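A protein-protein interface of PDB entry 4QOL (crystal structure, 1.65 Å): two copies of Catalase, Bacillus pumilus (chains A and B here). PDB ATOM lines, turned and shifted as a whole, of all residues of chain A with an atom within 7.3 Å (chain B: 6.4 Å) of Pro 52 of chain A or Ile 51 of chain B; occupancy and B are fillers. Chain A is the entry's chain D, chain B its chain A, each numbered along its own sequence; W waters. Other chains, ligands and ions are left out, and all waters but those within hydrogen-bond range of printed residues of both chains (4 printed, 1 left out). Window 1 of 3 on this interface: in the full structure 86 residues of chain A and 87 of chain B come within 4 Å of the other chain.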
ATOM      1  N   ARG A  50       8.963 -14.302 -11.293  1.00  0.00           N
ATOM      2  CA  ARG A  50      10.358 -14.536 -11.564  1.00  0.00           C
ATOM      3  C   ARG A  50      10.549 -15.833 -12.340  1.00  0.00           C
ATOM      4  O   ARG A  50       9.858 -16.838 -12.085  1.00  0.00           O
ATOM      5  CB  ARG A  50      11.214 -14.593 -10.282  1.00  0.00           C
ATOM      6  CG  ARG A  50      11.139 -13.385  -9.380  1.00  0.00           C
ATOM      7  CD  ARG A  50      11.717 -12.125  -9.985  1.00  0.00           C
ATOM      8  NE  ARG A  50      11.379 -11.025  -9.042  1.00  0.00           N
ATOM      9  CZ  ARG A  50      10.456 -10.097  -9.216  1.00  0.00           C
ATOM     10  NH1 ARG A  50       9.645 -10.044 -10.288  1.00  0.00           N
ATOM     11  NH2 ARG A  50      10.269  -9.278  -8.233  1.00  0.00           N
ATOM     12  N   ILE A  51      11.473 -15.736 -13.310  1.00  0.00           N
ATOM     13  CA  ILE A  51      12.001 -16.900 -14.045  1.00  0.00           C
ATOM     14  C   ILE A  51      13.529 -17.021 -13.775  1.00  0.00           C
ATOM     15  O   ILE A  51      14.134 -16.091 -13.235  1.00  0.00           O
ATOM     16  CB  ILE A  51      11.689 -16.740 -15.554  1.00  0.00           C
ATOM     17  CG1 ILE A  51      12.489 -15.579 -16.171  1.00  0.00           C
ATOM     18  CG2 ILE A  51      10.207 -16.546 -15.752  1.00  0.00           C
ATOM     19  CD1 ILE A  51      12.411 -15.513 -17.669  1.00  0.00           C
ATOM     20  N   PRO A  52      14.143 -18.181 -14.067  1.00  0.00           N
ATOM     21  CA  PRO A  52      15.550 -18.358 -13.754  1.00  0.00           C
ATOM     22  C   PRO A  52      16.339 -17.314 -14.521  1.00  0.00           C
ATOM     23  O   PRO A  52      15.963 -16.981 -15.628  1.00  0.00           O
ATOM     24  CB  PRO A  52      15.843 -19.796 -14.254  1.00  0.00           C
ATOM     25  CG  PRO A  52      14.523 -20.472 -14.345  1.00  0.00           C
ATOM     26  CD  PRO A  52      13.550 -19.363 -14.701  1.00  0.00           C
ATOM     27  N   GLU A  53      17.385 -16.777 -13.881  1.00  0.00           N
ATOM     28  CA  GLU A  53      18.310 -15.896 -14.542  1.00  0.00           C
ATOM     29  C   GLU A  53      19.194 -16.732 -15.475  1.00  0.00           C
ATOM     30  O   GLU A  53      19.270 -17.969 -15.351  1.00  0.00           O
ATOM     31  CB  GLU A  53      19.137 -15.033 -13.571  1.00  0.00           C
ATOM     32  CG  GLU A  53      20.281 -15.752 -12.910  1.00  0.00           C
ATOM     33  CD  GLU A  53      21.041 -14.948 -11.889  1.00  0.00           C
ATOM     34  OE1 GLU A  53      20.541 -13.875 -11.408  1.00  0.00           O
ATOM     35  OE2 GLU A  53      22.167 -15.415 -11.559  1.00  0.00           O
ATOM     36  N   ARG A  54      19.799 -16.047 -16.439  1.00  0.00           N
ATOM     37  CA  ARG A  54      20.737 -16.692 -17.315  1.00  0.00           C
ATOM     38  C   ARG A  54      21.887 -17.314 -16.498  1.00  0.00           C
ATOM     39  O   ARG A  54      22.350 -16.750 -15.540  1.00  0.00           O
ATOM     40  CB  ARG A  54      21.375 -15.687 -18.336  1.00  0.00           C
ATOM     41  CG  ARG A  54      20.400 -15.097 -19.288  1.00  0.00           C
ATOM     42  CD  ARG A  54      21.007 -13.826 -19.914  1.00  0.00           C
ATOM     43  NE  ARG A  54      20.184 -13.304 -21.009  1.00  0.00           N
ATOM     44  CZ  ARG A  54      19.044 -12.639 -20.856  1.00  0.00           C
ATOM     45  NH1 ARG A  54      18.546 -12.418 -19.652  1.00  0.00           N
ATOM     46  NH2 ARG A  54      18.362 -12.245 -21.918  1.00  0.00           N
ATOM     47  N   VAL A  55      22.299 -18.530 -16.883  1.00  0.00           N
ATOM     48  CA  VAL A  55      23.372 -19.243 -16.135  1.00  0.00           C
ATOM     49  C   VAL A  55      24.725 -18.538 -16.114  1.00  0.00           C
ATOM     50  O   VAL A  55      25.466 -18.612 -15.109  1.00  0.00           O
ATOM     51  CB  VAL A  55      23.487 -20.697 -16.683  1.00  0.00           C
ATOM     52  CG1 VAL A  55      24.014 -20.675 -18.106  1.00  0.00           C
ATOM     53  CG2 VAL A  55      24.333 -21.495 -15.755  1.00  0.00           C
ATOM     54  N   LYS A 102      22.068 -11.503 -11.503  1.00  0.00           N
ATOM     55  CA  LYS A 102      21.318 -10.382 -12.067  1.00  0.00           C
ATOM     56  C   LYS A 102      21.514  -8.996 -11.482  1.00  0.00           C
ATOM     57  O   LYS A 102      21.485  -8.014 -12.226  1.00  0.00           O
ATOM     58  CB  LYS A 102      19.816 -10.639 -11.925  1.00  0.00           C
ATOM     59  CG  LYS A 102      19.255 -11.142 -13.197  1.00  0.00           C
ATOM     60  CD  LYS A 102      17.746 -11.448 -13.088  1.00  0.00           C
ATOM     61  CE  LYS A 102      16.841 -10.201 -12.933  1.00  0.00           C
ATOM     62  NZ  LYS A 102      16.890  -9.263 -14.108  1.00  0.00           N
ATOM     63  N   PHE A 308      11.634  -6.666 -18.551  1.00  0.00           N
ATOM     64  CA  PHE A 308      11.478  -8.098 -18.453  1.00  0.00           C
ATOM     65  C   PHE A 308      11.134  -8.729 -19.776  1.00  0.00           C
ATOM     66  O   PHE A 308      11.723  -9.804 -20.139  1.00  0.00           O
ATOM     67  CB  PHE A 308      10.376  -8.480 -17.395  1.00  0.00           C
ATOM     68  CG  PHE A 308      10.130  -9.943 -17.277  1.00  0.00           C
ATOM     69  CD1 PHE A 308      10.910 -10.717 -16.415  1.00  0.00           C
ATOM     70  CD2 PHE A 308       9.163 -10.549 -18.049  1.00  0.00           C
ATOM     71  CE1 PHE A 308      10.703 -12.091 -16.338  1.00  0.00           C
ATOM     72  CE2 PHE A 308       8.923 -11.892 -17.961  1.00  0.00           C
ATOM     73  CZ  PHE A 308       9.734 -12.655 -17.111  1.00  0.00           C
ATOM     74  N   GLU A 312      15.039  -9.215 -20.496  1.00  0.00           N
ATOM     75  CA  GLU A 312      15.321 -10.357 -19.690  1.00  0.00           C
ATOM     76  C   GLU A 312      14.961 -11.631 -20.456  1.00  0.00           C
ATOM     77  O   GLU A 312      15.637 -12.637 -20.359  1.00  0.00           O
ATOM     78  CB  GLU A 312      14.518 -10.313 -18.344  1.00  0.00           C
ATOM     79  CG  GLU A 312      14.876 -11.487 -17.474  1.00  0.00           C
ATOM     80  CD  GLU A 312      16.300 -11.512 -16.967  1.00  0.00           C
ATOM     81  OE1 GLU A 312      16.791 -12.596 -16.548  1.00  0.00           O
ATOM     82  OE2 GLU A 312      16.897 -10.462 -16.822  1.00  0.00           O
ATOM     83  N   HIS A 346      14.715 -24.243 -21.166  1.00  0.00           N
ATOM     84  CA  HIS A 346      14.540 -24.316 -19.686  1.00  0.00           C
ATOM     85  C   HIS A 346      14.179 -22.984 -19.069  1.00  0.00           C
ATOM     86  O   HIS A 346      13.258 -22.857 -18.268  1.00  0.00           O
ATOM     87  CB  HIS A 346      15.831 -24.817 -19.068  1.00  0.00           C
ATOM     88  CG  HIS A 346      16.000 -24.459 -17.613  1.00  0.00           C
ATOM     89  ND1 HIS A 346      15.335 -25.106 -16.618  1.00  0.00           N
ATOM     90  CD2 HIS A 346      16.823 -23.568 -17.005  1.00  0.00           C
ATOM     91  CE1 HIS A 346      15.716 -24.620 -15.454  1.00  0.00           C
ATOM     92  NE2 HIS A 346      16.600 -23.663 -15.672  1.00  0.00           N
ATOM     93  N   ARG A 347      14.939 -21.949 -19.485  1.00  0.00           N
ATOM     94  CA  ARG A 347      14.830 -20.617 -18.835  1.00  0.00           C
ATOM     95  C   ARG A 347      13.510 -19.920 -19.221  1.00  0.00           C
ATOM     96  O   ARG A 347      12.930 -19.208 -18.417  1.00  0.00           O
ATOM     97  CB  ARG A 347      15.969 -19.721 -19.254  1.00  0.00           C
ATOM     98  CG  ARG A 347      16.029 -18.330 -18.671  1.00  0.00           C
ATOM     99  CD  ARG A 347      17.376 -17.659 -18.947  1.00  0.00           C
ATOM    100  NE  ARG A 347      17.687 -17.277 -20.316  1.00  0.00           N
ATOM    101  CZ  ARG A 347      17.252 -16.184 -20.960  1.00  0.00           C
ATOM    102  NH1 ARG A 347      16.369 -15.352 -20.350  1.00  0.00           N
ATOM    103  NH2 ARG A 347      17.701 -15.925 -22.214  1.00  0.00           N
ATOM    104  N   LEU A 348      13.061 -20.149 -20.467  1.00  0.00           N
ATOM    105  CA  LEU A 348      11.995 -19.368 -21.101  1.00  0.00           C
ATOM    106  C   LEU A 348      10.779 -20.128 -21.570  1.00  0.00           C
ATOM    107  O   LEU A 348       9.702 -19.549 -21.727  1.00  0.00           O
ATOM    108  CB  LEU A 348      12.588 -18.578 -22.316  1.00  0.00           C
ATOM    109  CG  LEU A 348      13.643 -17.538 -21.991  1.00  0.00           C
ATOM    110  CD1 LEU A 348      14.313 -17.161 -23.324  1.00  0.00           C
ATOM    111  CD2 LEU A 348      13.075 -16.329 -21.269  1.00  0.00           C
ATOM    112  N   ARG B  48      20.779 -25.993 -16.913  1.00  0.00           N
ATOM    113  CA  ARG B  48      19.605 -26.056 -16.026  1.00  0.00           C
ATOM    114  C   ARG B  48      19.929 -25.834 -14.549  1.00  0.00           C
ATOM    115  O   ARG B  48      19.080 -26.122 -13.713  1.00  0.00           O
ATOM    116  CB  ARG B  48      18.930 -27.417 -16.241  1.00  0.00           C
ATOM    117  CG  ARG B  48      18.189 -27.533 -17.544  1.00  0.00           C
ATOM    118  CD  ARG B  48      17.777 -28.928 -17.895  1.00  0.00           C
ATOM    119  NE  ARG B  48      17.147 -28.821 -19.167  1.00  0.00           N
ATOM    120  CZ  ARG B  48      17.816 -28.640 -20.339  1.00  0.00           C
ATOM    121  NH1 ARG B  48      19.076 -28.863 -20.351  1.00  0.00           N
ATOM    122  NH2 ARG B  48      17.152 -28.358 -21.438  1.00  0.00           N
ATOM    123  N   GLU B  49      21.091 -25.268 -14.212  1.00  0.00           N
ATOM    124  CA  GLU B  49      21.454 -25.037 -12.826  1.00  0.00           C
ATOM    125  C   GLU B  49      20.587 -24.056 -12.105  1.00  0.00           C
ATOM    126  O   GLU B  49      20.283 -24.263 -10.930  1.00  0.00           O
ATOM    127  CB  GLU B  49      22.869 -24.552 -12.668  1.00  0.00           C
ATOM    128  CG  GLU B  49      23.874 -25.631 -12.925  1.00  0.00           C
ATOM    129  CD  GLU B  49      25.308 -25.211 -12.729  1.00  0.00           C
ATOM    130  OE1 GLU B  49      26.201 -26.018 -13.168  1.00  0.00           O
ATOM    131  OE2 GLU B  49      25.617 -24.134 -12.134  1.00  0.00           O
ATOM    132  N   ARG B  50      20.070 -23.038 -12.815  1.00  0.00           N
ATOM    133  CA  ARG B  50      19.384 -21.944 -12.138  1.00  0.00           C
ATOM    134  C   ARG B  50      17.899 -22.193 -11.983  1.00  0.00           C
ATOM    135  O   ARG B  50      17.231 -22.725 -12.864  1.00  0.00           O
ATOM    136  CB  ARG B  50      19.608 -20.611 -12.973  1.00  0.00           C
ATOM    137  CG  ARG B  50      21.038 -20.196 -13.112  1.00  0.00           C
ATOM    138  CD  ARG B  50      21.779 -19.870 -11.828  1.00  0.00           C
ATOM    139  NE  ARG B  50      23.152 -19.670 -12.244  1.00  0.00           N
ATOM    140  CZ  ARG B  50      24.148 -20.529 -12.096  1.00  0.00           C
ATOM    141  NH1 ARG B  50      24.036 -21.725 -11.466  1.00  0.00           N
ATOM    142  NH2 ARG B  50      25.270 -20.243 -12.752  1.00  0.00           N
ATOM    143  N   ILE B  51      17.372 -21.713 -10.862  1.00  0.00           N
ATOM    144  CA  ILE B  51      15.945 -21.678 -10.612  1.00  0.00           C
ATOM    145  C   ILE B  51      15.541 -20.215 -10.299  1.00  0.00           C
ATOM    146  O   ILE B  51      16.429 -19.380 -10.042  1.00  0.00           O
ATOM    147  CB  ILE B  51      15.598 -22.603  -9.399  1.00  0.00           C
ATOM    148  CG1 ILE B  51      16.240 -22.117  -8.075  1.00  0.00           C
ATOM    149  CG2 ILE B  51      15.983 -24.036  -9.742  1.00  0.00           C
ATOM    150  CD1 ILE B  51      15.728 -22.879  -6.831  1.00  0.00           C
ATOM    151  N   PRO B  52      14.252 -19.931 -10.283  1.00  0.00           N
ATOM    152  CA  PRO B  52      13.897 -18.497 -10.048  1.00  0.00           C
ATOM    153  C   PRO B  52      14.367 -18.049  -8.690  1.00  0.00           C
ATOM    154  O   PRO B  52      14.330 -18.815  -7.764  1.00  0.00           O
ATOM    155  CB  PRO B  52      12.368 -18.450 -10.163  1.00  0.00           C
ATOM    156  CG  PRO B  52      12.005 -19.723 -10.913  1.00  0.00           C
ATOM    157  CD  PRO B  52      13.070 -20.742 -10.535  1.00  0.00           C
ATOM    158  N   GLU B  53      14.852 -16.828  -8.607  1.00  0.00           N
ATOM    159  CA  GLU B  53      15.141 -16.245  -7.305  1.00  0.00           C
ATOM    160  C   GLU B  53      13.839 -15.923  -6.586  1.00  0.00           C
ATOM    161  O   GLU B  53      12.769 -15.802  -7.200  1.00  0.00           O
ATOM    162  CB  GLU B  53      16.055 -14.988  -7.410  1.00  0.00           C
ATOM    163  CG  GLU B  53      15.353 -13.745  -7.852  1.00  0.00           C
ATOM    164  CD  GLU B  53      16.272 -12.547  -8.009  1.00  0.00           C
ATOM    165  OE1 GLU B  53      17.556 -12.691  -8.175  1.00  0.00           O
ATOM    166  OE2 GLU B  53      15.715 -11.379  -8.113  1.00  0.00           O
ATOM    167  N   LYS B 102      19.389 -11.231  -6.567  1.00  0.00           N
ATOM    168  CA  LYS B 102      20.613 -11.955  -6.199  1.00  0.00           C
ATOM    169  C   LYS B 102      21.804 -11.183  -6.748  1.00  0.00           C
ATOM    170  O   LYS B 102      21.748 -10.599  -7.811  1.00  0.00           O
ATOM    171  CB  LYS B 102      20.587 -13.374  -6.793  1.00  0.00           C
ATOM    172  CG  LYS B 102      19.694 -14.361  -6.032  1.00  0.00           C
ATOM    173  CD  LYS B 102      19.749 -15.712  -6.735  1.00  0.00           C
ATOM    174  CE  LYS B 102      21.123 -16.333  -6.669  1.00  0.00           C
ATOM    175  NZ  LYS B 102      21.471 -16.751  -5.273  1.00  0.00           N
ATOM    176  N   PHE B 308      23.475 -23.317  -2.509  1.00  0.00           N
ATOM    177  CA  PHE B 308      22.243 -23.511  -3.303  1.00  0.00           C
ATOM    178  C   PHE B 308      21.256 -24.464  -2.587  1.00  0.00           C
ATOM    179  O   PHE B 308      20.053 -24.184  -2.490  1.00  0.00           O
ATOM    180  CB  PHE B 308      22.579 -24.026  -4.698  1.00  0.00           C
ATOM    181  CG  PHE B 308      21.389 -24.319  -5.552  1.00  0.00           C
ATOM    182  CD1 PHE B 308      20.818 -23.343  -6.330  1.00  0.00           C
ATOM    183  CD2 PHE B 308      20.779 -25.564  -5.505  1.00  0.00           C
ATOM    184  CE1 PHE B 308      19.667 -23.636  -7.076  1.00  0.00           C
ATOM    185  CE2 PHE B 308      19.652 -25.866  -6.294  1.00  0.00           C
ATOM    186  CZ  PHE B 308      19.086 -24.917  -7.057  1.00  0.00           C
ATOM    187  N   GLU B 312      19.672 -21.296  -0.795  1.00  0.00           N
ATOM    188  CA  GLU B 312      18.855 -20.843  -1.908  1.00  0.00           C
ATOM    189  C   GLU B 312      17.519 -21.577  -1.905  1.00  0.00           C
ATOM    190  O   GLU B 312      16.492 -20.957  -2.146  1.00  0.00           O
ATOM    191  CB  GLU B 312      19.588 -20.932  -3.227  1.00  0.00           C
ATOM    192  CG  GLU B 312      18.778 -20.331  -4.353  1.00  0.00           C
ATOM    193  CD  GLU B 312      18.619 -18.807  -4.261  1.00  0.00           C
ATOM    194  OE1 GLU B 312      17.671 -18.298  -4.862  1.00  0.00           O
ATOM    195  OE2 GLU B 312      19.472 -18.143  -3.619  1.00  0.00           O
ATOM    196  N   GLN B 313      17.515 -22.872  -1.575  1.00  0.00           N
ATOM    197  CA  GLN B 313      16.278 -23.660  -1.645  1.00  0.00           C
ATOM    198  C   GLN B 313      15.449 -23.643  -0.297  1.00  0.00           C
ATOM    199  O   GLN B 313      14.432 -24.243  -0.274  1.00  0.00           O
ATOM    200  CB  GLN B 313      16.576 -25.133  -1.947  1.00  0.00           C
ATOM    201  CG  GLN B 313      16.941 -25.414  -3.402  1.00  0.00           C
ATOM    202  CD  GLN B 313      17.007 -26.872  -3.739  1.00  0.00           C
ATOM    203  OE1 GLN B 313      16.442 -27.305  -4.764  1.00  0.00           O
ATOM    204  NE2 GLN B 313      17.677 -27.625  -2.923  1.00  0.00           N
ATOM    205  N   ARG B 347       8.684 -21.726  -7.160  1.00  0.00           N
ATOM    206  CA  ARG B 347      10.099 -21.454  -7.174  1.00  0.00           C
ATOM    207  C   ARG B 347      10.891 -22.788  -7.081  1.00  0.00           C
ATOM    208  O   ARG B 347      11.966 -22.940  -7.666  1.00  0.00           O
ATOM    209  CB  ARG B 347      10.469 -20.563  -6.010  1.00  0.00           C
ATOM    210  CG  ARG B 347      11.927 -20.213  -5.871  1.00  0.00           C
ATOM    211  CD  ARG B 347      12.169 -19.056  -4.898  1.00  0.00           C
ATOM    212  NE  ARG B 347      11.872 -19.334  -3.472  1.00  0.00           N
ATOM    213  CZ  ARG B 347      12.698 -19.986  -2.637  1.00  0.00           C
ATOM    214  NH1 ARG B 347      13.879 -20.453  -3.102  1.00  0.00           N
ATOM    215  NH2 ARG B 347      12.377 -20.108  -1.346  1.00  0.00           N
ATOM    216  N   LEU B 348      10.357 -23.716  -6.296  1.00  0.00           N
ATOM    217  CA  LEU B 348      11.107 -24.920  -5.797  1.00  0.00           C
ATOM    218  C   LEU B 348      10.539 -26.284  -6.222  1.00  0.00           C
ATOM    219  O   LEU B 348      11.272 -27.254  -6.205  1.00  0.00           O
ATOM    220  CB  LEU B 348      11.217 -24.929  -4.280  1.00  0.00           C
ATOM    221  CG  LEU B 348      11.985 -23.753  -3.687  1.00  0.00           C
ATOM    222  CD1 LEU B 348      11.695 -23.738  -2.191  1.00  0.00           C
ATOM    223  CD2 LEU B 348      13.467 -23.866  -4.003  1.00  0.00           C
HETATM  224  O   HOH W   1      15.325 -15.131 -11.129  1.00  0.00           O
HETATM  225  O   HOH W   2      17.856 -17.298 -10.969  1.00  0.00           O
HETATM  226  O   HOH W   3      18.251 -14.370 -10.263  1.00  0.00           O
HETATM  227  O   HOH W   4      13.381 -10.771  -6.978  1.00  0.00           O
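NZ of Lys 102 of chain A is in salt-bridge range of OE2 of Glu 312 of chain A.
NZ of Lys 102 of chain B lies within salt-bridge range of OE2 of Glu 312 of chain B, at 2.9 Å.
OE2 of Glu 49 of chain B is in salt-bridge range of NH1 of Arg 50 of chain B, 3.0 Å away.
The side-chain carboxylate of Glu 53 of chain A lies within hydrogen-bond range of the backbone NH of Lys 102 of chain A (2.8 Å).
OE1 of Glu 53 of chain B sits at hydrogen-bond distance from N of Lys 102 of chain B (2.8 Å).
Water W1 lies within hydrogen-bond range of the backbone carbonyl oxygen (O) of Ile 51 of chain A (2.6 Å) and the backbone NH (N) of Glu 53 of chain B (3.1 Å).
Water W3 bridges OE1 of Glu 53 of chain A and OE1 of Glu 53 of chain B.
Water W4 bridges the side-chain carboxylate of Glu 53 of chain B (2.7 Å) and the guanidinium group of Arg 50 of chain A (2.9 Å).
Water W2 lies within hydrogen-bond range of the backbone carbonyl oxygen (O) of Ile 51 of chain B (2.7 Å) and the backbone NH (N) of Glu 53 of chain A (3.0 Å).
The backbone carbonyl oxygen of Val 55 of chain A is in hydrogen-bond range of the guanidinium group of Arg 50 of chain B (2.9 Å).
O of Arg 50 of chain B is in hydrogen-bond range of NE2 of His 346 of chain A (3.0 Å).
Arg 50 of chain A touches Pro 52 of chain B, and with the chains exchanged Pro 52 of chain A touches Arg 50 of chain B.
Arg 50 of chain A touches Glu 53 of chain B, and with the chains exchanged Glu 53 of chain A touches Arg 50 of chain B.
Pro 52 of chain A touches Ile 51 of chain B, but with the chains exchanged Ile 51 of chain A does not touch Pro 52 of chain B (4.0002 Å).
Lys 102 of chain B touches its own counterpart, Lys 102 of chain A.
Pro 52 of chain A touches just these residues of chain B: Arg 50 and Ile 51.
Printed residues of chain B within 4 Å of Val 55 of chain A: Arg 50 (2.9 Å).
Of chain A, only Pro 52 (3.9 Å) comes within 4 Å of Ile 51 of chain B.
Of the printed residues of chain A, Glu 53 of chain B touches Arg 50.
The nearest residue of chain B that does not touch Pro 52 of chain A is Pro 52 of chain B (4.03 Å).
The nearest residue of chain A that does not touch Ile 51 of chain B is Glu 53 of chain A (4.7 Å).
CB of Pro 52 of chain B touches O of Arg 50 of chain A, 3.5 Å away.
Arg 50 of chain A touches Glu 53 of chain B (CG to O, 3.6 Å).
Arg 50 of chain B touches Pro 52 of chain A (O to CB, 3.5 Å).
Pro 52 of chain A touches Ile 51 of chain B (CA to C, 3.9 Å).
Arg 50 of chain B touches Glu 53 of chain A (CB to O, 3.6 Å).
Lys 102 of chain A touches Lys 102 of chain B (N to O, 3.8 Å).
His 346 of chain A touches Arg 48 of chain B (CG to CG, 3.8 Å).
Of the 12 printed residues of chain B, 6 touch a printed residue of chain A.
Hydrophobic or aromatic side chains of chain B that line the printed part of chain A: Pro 52.
Among the printed residues, 9 pairs touch across the chains.
Among the printed residues, no Asp or Glu carboxylate lies within 4 Å of a Lys or Arg side-chain nitrogen of the other chain.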
